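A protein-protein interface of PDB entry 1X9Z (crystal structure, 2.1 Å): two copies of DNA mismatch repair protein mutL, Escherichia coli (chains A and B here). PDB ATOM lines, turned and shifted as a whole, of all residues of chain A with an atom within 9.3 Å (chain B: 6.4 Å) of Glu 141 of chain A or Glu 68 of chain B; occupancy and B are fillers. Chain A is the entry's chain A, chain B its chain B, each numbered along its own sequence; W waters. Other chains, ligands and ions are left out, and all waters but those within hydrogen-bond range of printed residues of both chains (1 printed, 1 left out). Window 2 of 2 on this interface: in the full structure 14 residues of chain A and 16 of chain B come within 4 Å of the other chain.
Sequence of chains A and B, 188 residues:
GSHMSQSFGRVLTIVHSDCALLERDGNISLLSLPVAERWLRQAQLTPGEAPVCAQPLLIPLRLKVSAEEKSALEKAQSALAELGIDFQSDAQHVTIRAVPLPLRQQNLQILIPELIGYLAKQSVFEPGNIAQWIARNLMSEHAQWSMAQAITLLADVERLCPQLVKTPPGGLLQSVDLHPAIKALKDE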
ATOM      1  N   PRO A  34      11.496 -10.172 -22.087  1.00  0.00           N
ATOM      2  CA  PRO A  34      12.897 -10.204 -21.627  1.00  0.00           C
ATOM      3  C   PRO A  34      13.542 -11.557 -21.936  1.00  0.00           C
ATOM      4  O   PRO A  34      14.709 -11.634 -22.317  1.00  0.00           O
ATOM      5  CB  PRO A  34      12.778  -9.967 -20.115  1.00  0.00           C
ATOM      6  CG  PRO A  34      11.517  -9.142 -19.993  1.00  0.00           C
ATOM      7  CD  PRO A  34      10.595  -9.873 -20.954  1.00  0.00           C
ATOM      8  N   GLU A  37      14.099 -11.651 -25.658  1.00  0.00           N
ATOM      9  CA  GLU A  37      15.219 -10.789 -26.017  1.00  0.00           C
ATOM     10  C   GLU A  37      16.534 -11.511 -25.716  1.00  0.00           C
ATOM     11  O   GLU A  37      17.478 -11.462 -26.486  1.00  0.00           O
ATOM     12  CB  GLU A  37      15.155  -9.478 -25.228  1.00  0.00           C
ATOM     13  CG  GLU A  37      16.304  -8.521 -25.518  1.00  0.00           C
ATOM     14  CD  GLU A  37      16.130  -7.717 -26.795  1.00  0.00           C
ATOM     15  OE1 GLU A  37      15.383  -8.150 -27.698  1.00  0.00           O
ATOM     16  OE2 GLU A  37      16.758  -6.641 -26.899  1.00  0.00           O
ATOM     17  N   ARG A  38      16.582 -12.189 -24.582  1.00  0.00           N
ATOM     18  CA  ARG A  38      17.773 -12.915 -24.200  1.00  0.00           C
ATOM     19  C   ARG A  38      18.132 -14.002 -25.238  1.00  0.00           C
ATOM     20  O   ARG A  38      19.288 -14.082 -25.685  1.00  0.00           O
ATOM     21  CB  ARG A  38      17.547 -13.521 -22.817  1.00  0.00           C
ATOM     22  CG  ARG A  38      18.645 -14.414 -22.296  1.00  0.00           C
ATOM     23  CD  ARG A  38      18.710 -14.275 -20.785  1.00  0.00           C
ATOM     24  NE  ARG A  38      17.377 -14.110 -20.204  1.00  0.00           N
ATOM     25  CZ  ARG A  38      17.074 -13.191 -19.294  1.00  0.00           C
ATOM     26  NH1 ARG A  38      18.009 -12.350 -18.862  1.00  0.00           N
ATOM     27  NH2 ARG A  38      15.840 -13.113 -18.814  1.00  0.00           N
ATOM     28  N   ARG A  41      19.569 -12.310 -28.316  1.00  0.00           N
ATOM     29  CA  ARG A  41      20.924 -11.810 -28.139  1.00  0.00           C
ATOM     30  C   ARG A  41      21.949 -12.924 -28.113  1.00  0.00           C
ATOM     31  O   ARG A  41      23.031 -12.791 -28.674  1.00  0.00           O
ATOM     32  CB  ARG A  41      21.017 -10.978 -26.857  1.00  0.00           C
ATOM     33  CG  ARG A  41      20.481  -9.557 -27.019  1.00  0.00           C
ATOM     34  CD  ARG A  41      20.274  -8.898 -25.659  1.00  0.00           C
ATOM     35  NE  ARG A  41      20.007  -7.466 -25.766  1.00  0.00           N
ATOM     36  CZ  ARG A  41      19.619  -6.702 -24.749  1.00  0.00           C
ATOM     37  NH1 ARG A  41      19.447  -7.231 -23.539  1.00  0.00           N
ATOM     38  NH2 ARG A  41      19.407  -5.407 -24.940  1.00  0.00           N
ATOM     39  N   GLN A 105      26.154  -0.651 -29.231  1.00  0.00           N
ATOM     40  CA  GLN A 105      25.359   0.385 -28.580  1.00  0.00           C
ATOM     41  C   GLN A 105      25.116   0.180 -27.081  1.00  0.00           C
ATOM     42  O   GLN A 105      24.289   0.864 -26.480  1.00  0.00           O
ATOM     43  CB  GLN A 105      24.006   0.544 -29.295  1.00  0.00           C
ATOM     44  CG  GLN A 105      24.142   0.925 -30.767  1.00  0.00           C
ATOM     45  CD  GLN A 105      24.954   2.198 -30.972  1.00  0.00           C
ATOM     46  OE1 GLN A 105      25.581   2.388 -32.016  1.00  0.00           O
ATOM     47  NE2 GLN A 105      24.940   3.078 -29.977  1.00  0.00           N
ATOM     48  N   GLN A 106      25.808  -0.773 -26.478  1.00  0.00           N
ATOM     49  CA  GLN A 106      25.650  -0.996 -25.051  1.00  0.00           C
ATOM     50  C   GLN A 106      26.568   0.002 -24.361  1.00  0.00           C
ATOM     51  O   GLN A 106      27.403   0.628 -25.017  1.00  0.00           O
ATOM     52  CB  GLN A 106      26.085  -2.422 -24.684  1.00  0.00           C
ATOM     53  CG  GLN A 106      25.145  -3.492 -25.181  1.00  0.00           C
ATOM     54  CD  GLN A 106      23.789  -3.371 -24.524  1.00  0.00           C
ATOM     55  OE1 GLN A 106      23.656  -3.574 -23.316  1.00  0.00           O
ATOM     56  NE2 GLN A 106      22.773  -3.021 -25.313  1.00  0.00           N
ATOM     57  N   ASN A 107      26.422   0.150 -23.051  1.00  0.00           N
ATOM     58  CA  ASN A 107      27.296   1.048 -22.301  1.00  0.00           C
ATOM     59  C   ASN A 107      28.529   0.211 -21.929  1.00  0.00           C
ATOM     60  O   ASN A 107      28.564  -0.457 -20.887  1.00  0.00           O
ATOM     61  CB  ASN A 107      26.587   1.561 -21.041  1.00  0.00           C
ATOM     62  CG  ASN A 107      27.520   2.341 -20.130  1.00  0.00           C
ATOM     63  OD1 ASN A 107      28.569   2.815 -20.564  1.00  0.00           O
ATOM     64  ND2 ASN A 107      27.142   2.480 -18.866  1.00  0.00           N
ATOM     65  N   ILE A 110      30.541  -0.134 -18.500  1.00  0.00           N
ATOM     66  CA  ILE A 110      30.020  -1.007 -17.472  1.00  0.00           C
ATOM     67  C   ILE A 110      30.068  -2.464 -17.969  1.00  0.00           C
ATOM     68  O   ILE A 110      30.479  -3.371 -17.232  1.00  0.00           O
ATOM     69  CB  ILE A 110      28.551  -0.649 -17.107  1.00  0.00           C
ATOM     70  CG1 ILE A 110      28.474   0.780 -16.538  1.00  0.00           C
ATOM     71  CG2 ILE A 110      28.018  -1.638 -16.101  1.00  0.00           C
ATOM     72  CD1 ILE A 110      29.265   1.012 -15.235  1.00  0.00           C
ATOM     73  N   LEU A 111      29.647  -2.708 -19.211  1.00  0.00           N
ATOM     74  CA  LEU A 111      29.656  -4.073 -19.743  1.00  0.00           C
ATOM     75  C   LEU A 111      31.043  -4.736 -19.822  1.00  0.00           C
ATOM     76  O   LEU A 111      31.211  -5.843 -19.360  1.00  0.00           O
ATOM     77  CB  LEU A 111      28.990  -4.120 -21.128  1.00  0.00           C
ATOM     78  CG  LEU A 111      29.232  -5.384 -21.963  1.00  0.00           C
ATOM     79  CD1 LEU A 111      28.434  -6.500 -21.405  1.00  0.00           C
ATOM     80  CD2 LEU A 111      28.817  -5.163 -23.395  1.00  0.00           C
ATOM     81  N   GLU A 114      32.510  -5.657 -16.616  1.00  0.00           N
ATOM     82  CA  GLU A 114      31.731  -6.777 -16.109  1.00  0.00           C
ATOM     83  C   GLU A 114      32.175  -8.076 -16.766  1.00  0.00           C
ATOM     84  O   GLU A 114      32.290  -9.111 -16.100  1.00  0.00           O
ATOM     85  CB  GLU A 114      30.249  -6.557 -16.356  1.00  0.00           C
ATOM     86  CG  GLU A 114      29.584  -5.555 -15.418  1.00  0.00           C
ATOM     87  CD  GLU A 114      28.095  -5.470 -15.675  1.00  0.00           C
ATOM     88  OE1 GLU A 114      27.711  -5.044 -16.777  1.00  0.00           O
ATOM     89  OE2 GLU A 114      27.308  -5.849 -14.791  1.00  0.00           O
ATOM     90  N   ALA A 135      24.730 -12.480 -22.923  1.00  0.00           N
ATOM     91  CA  ALA A 135      23.318 -12.332 -23.249  1.00  0.00           C
ATOM     92  C   ALA A 135      22.429 -12.292 -22.010  1.00  0.00           C
ATOM     93  O   ALA A 135      21.541 -11.451 -21.907  1.00  0.00           O
ATOM     94  CB  ALA A 135      22.873 -13.456 -24.198  1.00  0.00           C
ATOM     95  N   ARG A 136      22.683 -13.182 -21.058  1.00  0.00           N
ATOM     96  CA  ARG A 136      21.874 -13.238 -19.846  1.00  0.00           C
ATOM     97  C   ARG A 136      22.088 -12.150 -18.803  1.00  0.00           C
ATOM     98  O   ARG A 136      21.124 -11.600 -18.269  1.00  0.00           O
ATOM     99  CB  ARG A 136      22.077 -14.561 -19.114  1.00  0.00           C
ATOM    100  CG  ARG A 136      21.673 -15.815 -19.835  1.00  0.00           C
ATOM    101  CD  ARG A 136      21.649 -16.924 -18.804  1.00  0.00           C
ATOM    102  NE  ARG A 136      21.509 -18.254 -19.380  1.00  0.00           N
ATOM    103  CZ  ARG A 136      21.542 -19.372 -18.659  1.00  0.00           C
ATOM    104  NH1 ARG A 136      21.710 -19.308 -17.340  1.00  0.00           N
ATOM    105  NH2 ARG A 136      21.410 -20.553 -19.250  1.00  0.00           N
ATOM    106  N   ASN A 137      23.342 -11.838 -18.509  1.00  0.00           N
ATOM    107  CA  ASN A 137      23.637 -10.898 -17.432  1.00  0.00           C
ATOM    108  C   ASN A 137      24.070  -9.480 -17.712  1.00  0.00           C
ATOM    109  O   ASN A 137      23.661  -8.558 -17.017  1.00  0.00           O
ATOM    110  CB  ASN A 137      24.704 -11.502 -16.501  1.00  0.00           C
ATOM    111  CG  ASN A 137      24.313 -12.872 -15.945  1.00  0.00           C
ATOM    112  OD1 ASN A 137      24.650 -13.919 -16.510  1.00  0.00           O
ATOM    113  ND2 ASN A 137      23.597 -12.865 -14.824  1.00  0.00           N
ATOM    114  N   LEU A 138      24.904  -9.289 -18.715  1.00  0.00           N
ATOM    115  CA  LEU A 138      25.446  -7.967 -18.946  1.00  0.00           C
ATOM    116  C   LEU A 138      24.718  -6.978 -19.809  1.00  0.00           C
ATOM    117  O   LEU A 138      25.118  -5.811 -19.867  1.00  0.00           O
ATOM    118  CB  LEU A 138      26.864  -8.095 -19.494  1.00  0.00           C
ATOM    119  CG  LEU A 138      27.863  -8.886 -18.657  1.00  0.00           C
ATOM    120  CD1 LEU A 138      29.269  -8.786 -19.258  1.00  0.00           C
ATOM    121  CD2 LEU A 138      27.830  -8.345 -17.240  1.00  0.00           C
ATOM    122  N   MET A 139      23.642  -7.380 -20.456  1.00  0.00           N
ATOM    123  CA  MET A 139      23.051  -6.418 -21.351  1.00  0.00           C
ATOM    124  C   MET A 139      21.979  -5.436 -20.923  1.00  0.00           C
ATOM    125  O   MET A 139      21.295  -5.592 -19.911  1.00  0.00           O
ATOM    126  CB  MET A 139      22.664  -7.132 -22.645  1.00  0.00           C
ATOM    127  CG  MET A 139      23.922  -7.648 -23.334  1.00  0.00           C
ATOM    128  SD  MET A 139      23.733  -8.083 -25.173  1.00  0.00           S
ATOM    129  CE  MET A 139      23.519  -9.971 -25.022  1.00  0.00           C
ATOM    130  N   SER A 140      21.921  -4.378 -21.718  1.00  0.00           N
ATOM    131  CA  SER A 140      20.994  -3.284 -21.558  1.00  0.00           C
ATOM    132  C   SER A 140      19.662  -3.771 -21.048  1.00  0.00           C
ATOM    133  O   SER A 140      18.992  -4.594 -21.673  1.00  0.00           O
ATOM    134  CB  SER A 140      20.790  -2.586 -22.900  1.00  0.00           C
ATOM    135  OG  SER A 140      19.749  -1.643 -22.821  1.00  0.00           O
ATOM    136  N   GLU A 141      19.289  -3.256 -19.890  1.00  0.00           N
ATOM    137  CA  GLU A 141      18.022  -3.591 -19.289  1.00  0.00           C
ATOM    138  C   GLU A 141      16.997  -2.970 -20.240  1.00  0.00           C
ATOM    139  O   GLU A 141      17.362  -2.208 -21.133  1.00  0.00           O
ATOM    140  CB  GLU A 141      17.945  -2.947 -17.901  1.00  0.00           C
ATOM    141  CG  GLU A 141      19.287  -2.966 -17.142  1.00  0.00           C
ATOM    142  CD  GLU A 141      20.305  -1.928 -17.652  1.00  0.00           C
ATOM    143  OE1 GLU A 141      20.112  -0.718 -17.413  1.00  0.00           O
ATOM    144  OE2 GLU A 141      21.304  -2.315 -18.292  1.00  0.00           O
ATOM    145  N   HIS A 142      15.722  -3.291 -20.072  1.00  0.00           N
ATOM    146  CA  HIS A 142      14.717  -2.709 -20.951  1.00  0.00           C
ATOM    147  C   HIS A 142      13.560  -2.140 -20.143  1.00  0.00           C
ATOM    148  O   HIS A 142      13.047  -2.790 -19.229  1.00  0.00           O
ATOM    149  CB  HIS A 142      14.187  -3.755 -21.946  1.00  0.00           C
ATOM    150  CG  HIS A 142      13.420  -3.161 -23.090  1.00  0.00           C
ATOM    151  ND1 HIS A 142      12.303  -2.374 -22.912  1.00  0.00           N
ATOM    152  CD2 HIS A 142      13.628  -3.215 -24.428  1.00  0.00           C
ATOM    153  CE1 HIS A 142      11.858  -1.965 -24.087  1.00  0.00           C
ATOM    154  NE2 HIS A 142      12.646  -2.462 -25.023  1.00  0.00           N
ATOM    155  N   ALA A 143      13.156  -0.918 -20.478  1.00  0.00           N
ATOM    156  CA  ALA A 143      12.040  -0.284 -19.792  1.00  0.00           C
ATOM    157  C   ALA A 143      10.739  -0.847 -20.354  1.00  0.00           C
ATOM    158  O   ALA A 143      10.670  -2.016 -20.749  1.00  0.00           O
ATOM    159  CB  ALA A 143      12.080   1.229 -19.995  1.00  0.00           C
ATOM    160  N   GLN A 144       9.716  -0.004 -20.388  1.00  0.00           N
ATOM    161  CA  GLN A 144       8.401  -0.371 -20.893  1.00  0.00           C
ATOM    162  C   GLN A 144       8.460  -0.859 -22.344  1.00  0.00           C
ATOM    163  O   GLN A 144       9.045  -0.200 -23.201  1.00  0.00           O
ATOM    164  CB  GLN A 144       7.474   0.843 -20.816  1.00  0.00           C
ATOM    165  CG  GLN A 144       6.089   0.604 -21.383  1.00  0.00           C
ATOM    166  CD  GLN A 144       5.288  -0.348 -20.522  1.00  0.00           C
ATOM    167  OE1 GLN A 144       4.654  -1.284 -21.026  1.00  0.00           O
ATOM    168  NE2 GLN A 144       5.307  -0.114 -19.215  1.00  0.00           N
ATOM    169  N   TRP A 145       7.850  -2.012 -22.614  1.00  0.00           N
ATOM    170  CA  TRP A 145       7.822  -2.542 -23.974  1.00  0.00           C
ATOM    171  C   TRP A 145       6.617  -2.021 -24.760  1.00  0.00           C
ATOM    172  O   TRP A 145       5.538  -1.804 -24.202  1.00  0.00           O
ATOM    173  CB  TRP A 145       7.786  -4.070 -23.959  1.00  0.00           C
ATOM    174  CG  TRP A 145       9.104  -4.702 -23.596  1.00  0.00           C
ATOM    175  CD1 TRP A 145       9.615  -4.870 -22.346  1.00  0.00           C
ATOM    176  CD2 TRP A 145      10.070  -5.257 -24.505  1.00  0.00           C
ATOM    177  NE1 TRP A 145      10.835  -5.500 -22.413  1.00  0.00           N
ATOM    178  CE2 TRP A 145      11.140  -5.746 -23.724  1.00  0.00           C
ATOM    179  CE3 TRP A 145      10.133  -5.386 -25.901  1.00  0.00           C
ATOM    180  CZ2 TRP A 145      12.268  -6.362 -24.296  1.00  0.00           C
ATOM    181  CZ3 TRP A 145      11.256  -5.999 -26.471  1.00  0.00           C
ATOM    182  CH2 TRP A 145      12.307  -6.474 -25.667  1.00  0.00           C
ATOM    183  N   GLN A 149       7.964  -2.791 -30.686  1.00  0.00           N
ATOM    184  CA  GLN A 149       9.153  -3.479 -30.222  1.00  0.00           C
ATOM    185  C   GLN A 149       8.907  -4.979 -30.076  1.00  0.00           C
ATOM    186  O   GLN A 149       9.757  -5.784 -30.459  1.00  0.00           O
ATOM    187  CB  GLN A 149       9.635  -2.897 -28.883  1.00  0.00           C
ATOM    188  CG  GLN A 149      10.068  -1.426 -28.949  1.00  0.00           C
ATOM    189  CD  GLN A 149      10.309  -0.827 -27.567  1.00  0.00           C
ATOM    190  OE1 GLN A 149       9.781  -1.316 -26.566  1.00  0.00           O
ATOM    191  NE2 GLN A 149      11.092   0.249 -27.512  1.00  0.00           N
ATOM    192  N   VAL B  65      27.197   6.068 -17.056  1.00  0.00           N
ATOM    193  CA  VAL B  65      26.061   5.194 -16.782  1.00  0.00           C
ATOM    194  C   VAL B  65      24.869   5.517 -17.679  1.00  0.00           C
ATOM    195  O   VAL B  65      24.685   6.650 -18.117  1.00  0.00           O
ATOM    196  CB  VAL B  65      25.564   5.312 -15.306  1.00  0.00           C
ATOM    197  CG1 VAL B  65      26.604   4.743 -14.349  1.00  0.00           C
ATOM    198  CG2 VAL B  65      25.265   6.770 -14.975  1.00  0.00           C
ATOM    199  N   SER B  66      24.047   4.510 -17.932  1.00  0.00           N
ATOM    200  CA  SER B  66      22.869   4.686 -18.756  1.00  0.00           C
ATOM    201  C   SER B  66      21.757   5.202 -17.856  1.00  0.00           C
ATOM    202  O   SER B  66      21.826   5.054 -16.631  1.00  0.00           O
ATOM    203  CB  SER B  66      22.448   3.351 -19.352  1.00  0.00           C
ATOM    204  OG  SER B  66      21.937   2.507 -18.337  1.00  0.00           O
ATOM    205  N   ALA B  67      20.733   5.799 -18.462  1.00  0.00           N
ATOM    206  CA  ALA B  67      19.601   6.321 -17.710  1.00  0.00           C
ATOM    207  C   ALA B  67      19.110   5.275 -16.720  1.00  0.00           C
ATOM    208  O   ALA B  67      18.833   5.585 -15.566  1.00  0.00           O
ATOM    209  CB  ALA B  67      18.465   6.704 -18.662  1.00  0.00           C
ATOM    210  N   GLU B  68      19.003   4.036 -17.178  1.00  0.00           N
ATOM    211  CA  GLU B  68      18.534   2.952 -16.327  1.00  0.00           C
ATOM    212  C   GLU B  68      19.495   2.658 -15.169  1.00  0.00           C
ATOM    213  O   GLU B  68      19.064   2.302 -14.073  1.00  0.00           O
ATOM    214  CB  GLU B  68      18.329   1.690 -17.170  1.00  0.00           C
ATOM    215  CG  GLU B  68      17.643   0.536 -16.435  1.00  0.00           C
ATOM    216  CD  GLU B  68      16.203   0.850 -16.047  1.00  0.00           C
ATOM    217  OE1 GLU B  68      15.678   1.905 -16.486  1.00  0.00           O
ATOM    218  OE2 GLU B  68      15.597   0.034 -15.310  1.00  0.00           O
ATOM    219  N   GLU B  69      20.796   2.799 -15.415  1.00  0.00           N
ATOM    220  CA  GLU B  69      21.800   2.546 -14.382  1.00  0.00           C
ATOM    221  C   GLU B  69      21.774   3.725 -13.430  1.00  0.00           C
ATOM    222  O   GLU B  69      21.825   3.562 -12.212  1.00  0.00           O
ATOM    223  CB  GLU B  69      23.191   2.396 -15.009  1.00  0.00           C
ATOM    224  CG  GLU B  69      23.248   1.282 -16.035  1.00  0.00           C
ATOM    225  CD  GLU B  69      24.570   1.194 -16.785  1.00  0.00           C
ATOM    226  OE1 GLU B  69      25.259   2.221 -16.961  1.00  0.00           O
ATOM    227  OE2 GLU B  69      24.907   0.081 -17.227  1.00  0.00           O
ATOM    228  N   LYS B  70      21.683   4.911 -14.020  1.00  0.00           N
ATOM    229  CA  LYS B  70      21.621   6.168 -13.293  1.00  0.00           C
ATOM    230  C   LYS B  70      20.460   6.111 -12.322  1.00  0.00           C
ATOM    231  O   LYS B  70      20.596   6.438 -11.146  1.00  0.00           O
ATOM    232  CB  LYS B  70      21.389   7.317 -14.276  1.00  0.00           C
ATOM    233  CG  LYS B  70      21.248   8.688 -13.628  1.00  0.00           C
ATOM    234  CD  LYS B  70      22.578   9.215 -13.118  1.00  0.00           C
ATOM    235  CE  LYS B  70      22.422  10.620 -12.546  1.00  0.00           C
ATOM    236  NZ  LYS B  70      21.931  11.594 -13.567  1.00  0.00           N
ATOM    237  N   SER B  71      19.313   5.690 -12.839  1.00  0.00           N
ATOM    238  CA  SER B  71      18.092   5.594 -12.055  1.00  0.00           C
ATOM    239  C   SER B  71      18.223   4.598 -10.923  1.00  0.00           C
ATOM    240  O   SER B  71      17.868   4.897  -9.782  1.00  0.00           O
ATOM    241  CB  SER B  71      16.918   5.190 -12.957  1.00  0.00           C
ATOM    242  OG  SER B  71      15.765   4.864 -12.194  1.00  0.00           O
ATOM    243  N   ALA B  72      18.708   3.403 -11.247  1.00  0.00           N
ATOM    244  CA  ALA B  72      18.881   2.359 -10.242  1.00  0.00           C
ATOM    245  C   ALA B  72      19.779   2.872  -9.110  1.00  0.00           C
ATOM    246  O   ALA B  72      19.468   2.685  -7.928  1.00  0.00           O
ATOM    247  CB  ALA B  72      19.489   1.119 -10.878  1.00  0.00           C
ATOM    248  N   LEU B  73      20.879   3.534  -9.470  1.00  0.00           N
ATOM    249  CA  LEU B  73      21.792   4.055  -8.465  1.00  0.00           C
ATOM    250  C   LEU B  73      21.074   5.037  -7.548  1.00  0.00           C
ATOM    251  O   LEU B  73      21.265   5.008  -6.331  1.00  0.00           O
ATOM    252  CB  LEU B  73      23.002   4.723  -9.131  1.00  0.00           C
ATOM    253  CG  LEU B  73      24.072   3.736  -9.629  1.00  0.00           C
ATOM    254  CD1 LEU B  73      25.150   4.445 -10.454  1.00  0.00           C
ATOM    255  CD2 LEU B  73      24.681   3.045  -8.414  1.00  0.00           C
ATOM    256  N   LYS B  75      17.888   5.178  -6.684  1.00  0.00           N
ATOM    257  CA  LYS B  75      17.050   4.451  -5.735  1.00  0.00           C
ATOM    258  C   LYS B  75      17.844   3.719  -4.644  1.00  0.00           C
ATOM    259  O   LYS B  75      17.348   3.544  -3.531  1.00  0.00           O
ATOM    260  CB  LYS B  75      16.197   3.416  -6.471  1.00  0.00           C
ATOM    261  CG  LYS B  75      15.252   3.971  -7.518  1.00  0.00           C
ATOM    262  CD  LYS B  75      14.507   2.823  -8.164  1.00  0.00           C
ATOM    263  CE  LYS B  75      13.603   3.292  -9.274  1.00  0.00           C
ATOM    264  NZ  LYS B  75      13.010   2.124  -9.985  1.00  0.00           N
ATOM    265  N   GLY B 117      25.816  -3.013 -12.502  1.00  0.00           N
ATOM    266  CA  GLY B 117      25.057  -3.938 -13.326  1.00  0.00           C
ATOM    267  C   GLY B 117      24.056  -4.691 -12.469  1.00  0.00           C
ATOM    268  O   GLY B 117      22.900  -4.914 -12.859  1.00  0.00           O
ATOM    269  N   LEU B 119      22.771  -3.680  -9.535  1.00  0.00           N
ATOM    270  CA  LEU B 119      21.730  -2.774  -9.078  1.00  0.00           C
ATOM    271  C   LEU B 119      20.717  -2.422 -10.175  1.00  0.00           C
ATOM    272  O   LEU B 119      19.539  -2.226  -9.892  1.00  0.00           O
ATOM    273  CB  LEU B 119      22.348  -1.495  -8.510  1.00  0.00           C
ATOM    274  CG  LEU B 119      23.208  -1.627  -7.253  1.00  0.00           C
ATOM    275  CD1 LEU B 119      23.826  -0.274  -6.935  1.00  0.00           C
ATOM    276  CD2 LEU B 119      22.351  -2.093  -6.082  1.00  0.00           C
ATOM    277  N   ALA B 120      21.164  -2.365 -11.421  1.00  0.00           N
ATOM    278  CA  ALA B 120      20.257  -2.026 -12.506  1.00  0.00           C
ATOM    279  C   ALA B 120      19.175  -3.078 -12.723  1.00  0.00           C
ATOM    280  O   ALA B 120      18.198  -2.825 -13.424  1.00  0.00           O
ATOM    281  CB  ALA B 120      21.035  -1.834 -13.787  1.00  0.00           C
ATOM    282  N   LYS B 121      19.335  -4.253 -12.133  1.00  0.00           N
ATOM    283  CA  LYS B 121      18.341  -5.300 -12.320  1.00  0.00           C
ATOM    284  C   LYS B 121      17.449  -5.529 -11.099  1.00  0.00           C
ATOM    285  O   LYS B 121      16.559  -6.379 -11.125  1.00  0.00           O
ATOM    286  CB  LYS B 121      19.034  -6.606 -12.729  1.00  0.00           C
ATOM    287  CG  LYS B 121      19.804  -6.479 -14.046  1.00  0.00           C
ATOM    288  CD  LYS B 121      20.527  -7.766 -14.452  1.00  0.00           C
ATOM    289  CE  LYS B 121      21.602  -8.156 -13.449  1.00  0.00           C
ATOM    290  NZ  LYS B 121      22.578  -9.113 -14.044  1.00  0.00           N
HETATM  291  O   HOH W   1      21.341 -11.224 -14.034  1.00  0.00           O
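ND2 of Asn 107 of chain A is in hydrogen-bond range of OE1 of Glu 69 of chain B (2.7 Å). The backbone carbonyl oxygen (O) of Asn 137 of chain A is in hydrogen-bond range of the side-chain amino group (NZ) of Lys 121 of chain B.
The backbone NH (N) of Ser 66 of chain B lies within hydrogen-bond range of the side-chain carboxylate (OE1) of Glu 69 of chain B (2.8 Å).
ND2 of Asn 107 of chain A touches CA of Val 65 of chain B (3.6 Å). Ser 66 of chain B touches Asn 107 of chain A (N to ND2, 3.8 Å). Ile 110 of chain A touches Glu 69 of chain B (CG1 to OE1, 3.5 Å). Glu 114 of chain A touches Gly 117 of chain B (OE2 to CA, 3.3 Å). Glu 141 of chain A touches Ser 66 of chain B. OE1 of Glu 141 of chain A touches CG of Glu 68 of chain B, 2.9 Å away. CG of Glu 69 of chain B touches OE1 of Glu 141 of chain A (3.97 Å). O of Ala 120 of chain B touches CG of Glu 141 of chain A, at 3.9 Å.
Of chain B, only Ser 66, Glu 68, Glu 69 and Ala 120 come within 4 Å of Glu 141 of chain A. Gln 144 of chain A touches none of the printed residues of chain B. Of the printed residues of chain A, Val 65 of chain B touches Asn 107 (3.6 Å). Of chain A, only Asn 107 and Glu 141 come within 4 Å of Ser 66 of chain B. Of chain A, only Glu 141 (2.9 Å) comes within 4 Å of Glu 68 of chain B. Of the printed residues of chain A, Glu 69 of chain B touches Asn 107, Ile 110 and Glu 141. No residue of chain A comes within 4 Å of Ser 71 of chain B. Of the printed residues of chain A, Ala 120 of chain B touches Glu 141 (3.9 Å). Printed residues of chain A within 4 Å of Lys 121 of chain B: Asn 137. The nearest residue of chain A that does not touch Glu 68 of chain B is Ala 143 of chain A (5.1 Å). The nearest printed residue of chain A that does not touch Lys 121 of chain B is Glu 141 of chain A (4.7 Å).
Hydrophobic or aromatic side chains of chain B that line the printed part of chain A: Ala 120. Hydrophobic or aromatic side chains of chain A within 4 Å of the printed part of chain B: Ile 110. Along chain A the printed residues that touch a printed residue of chain B span positions 107 to 141. Among the printed residues, 10 pairs touch across the chains. Among the printed residues, no Asp or Glu carboxylate lies within 4 Å of a Lys or Arg side-chain nitrogen of the other chain.
No position is printed for both chains. Of the 10 pairs that touch across the chains among the printed residues, none has its exchanged pair printed and touching as well.
Water W1 bridges NZ of Lys 121 of chain B (2.4 Å) and ND2 of Asn 137 of chain A (2.9 Å).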
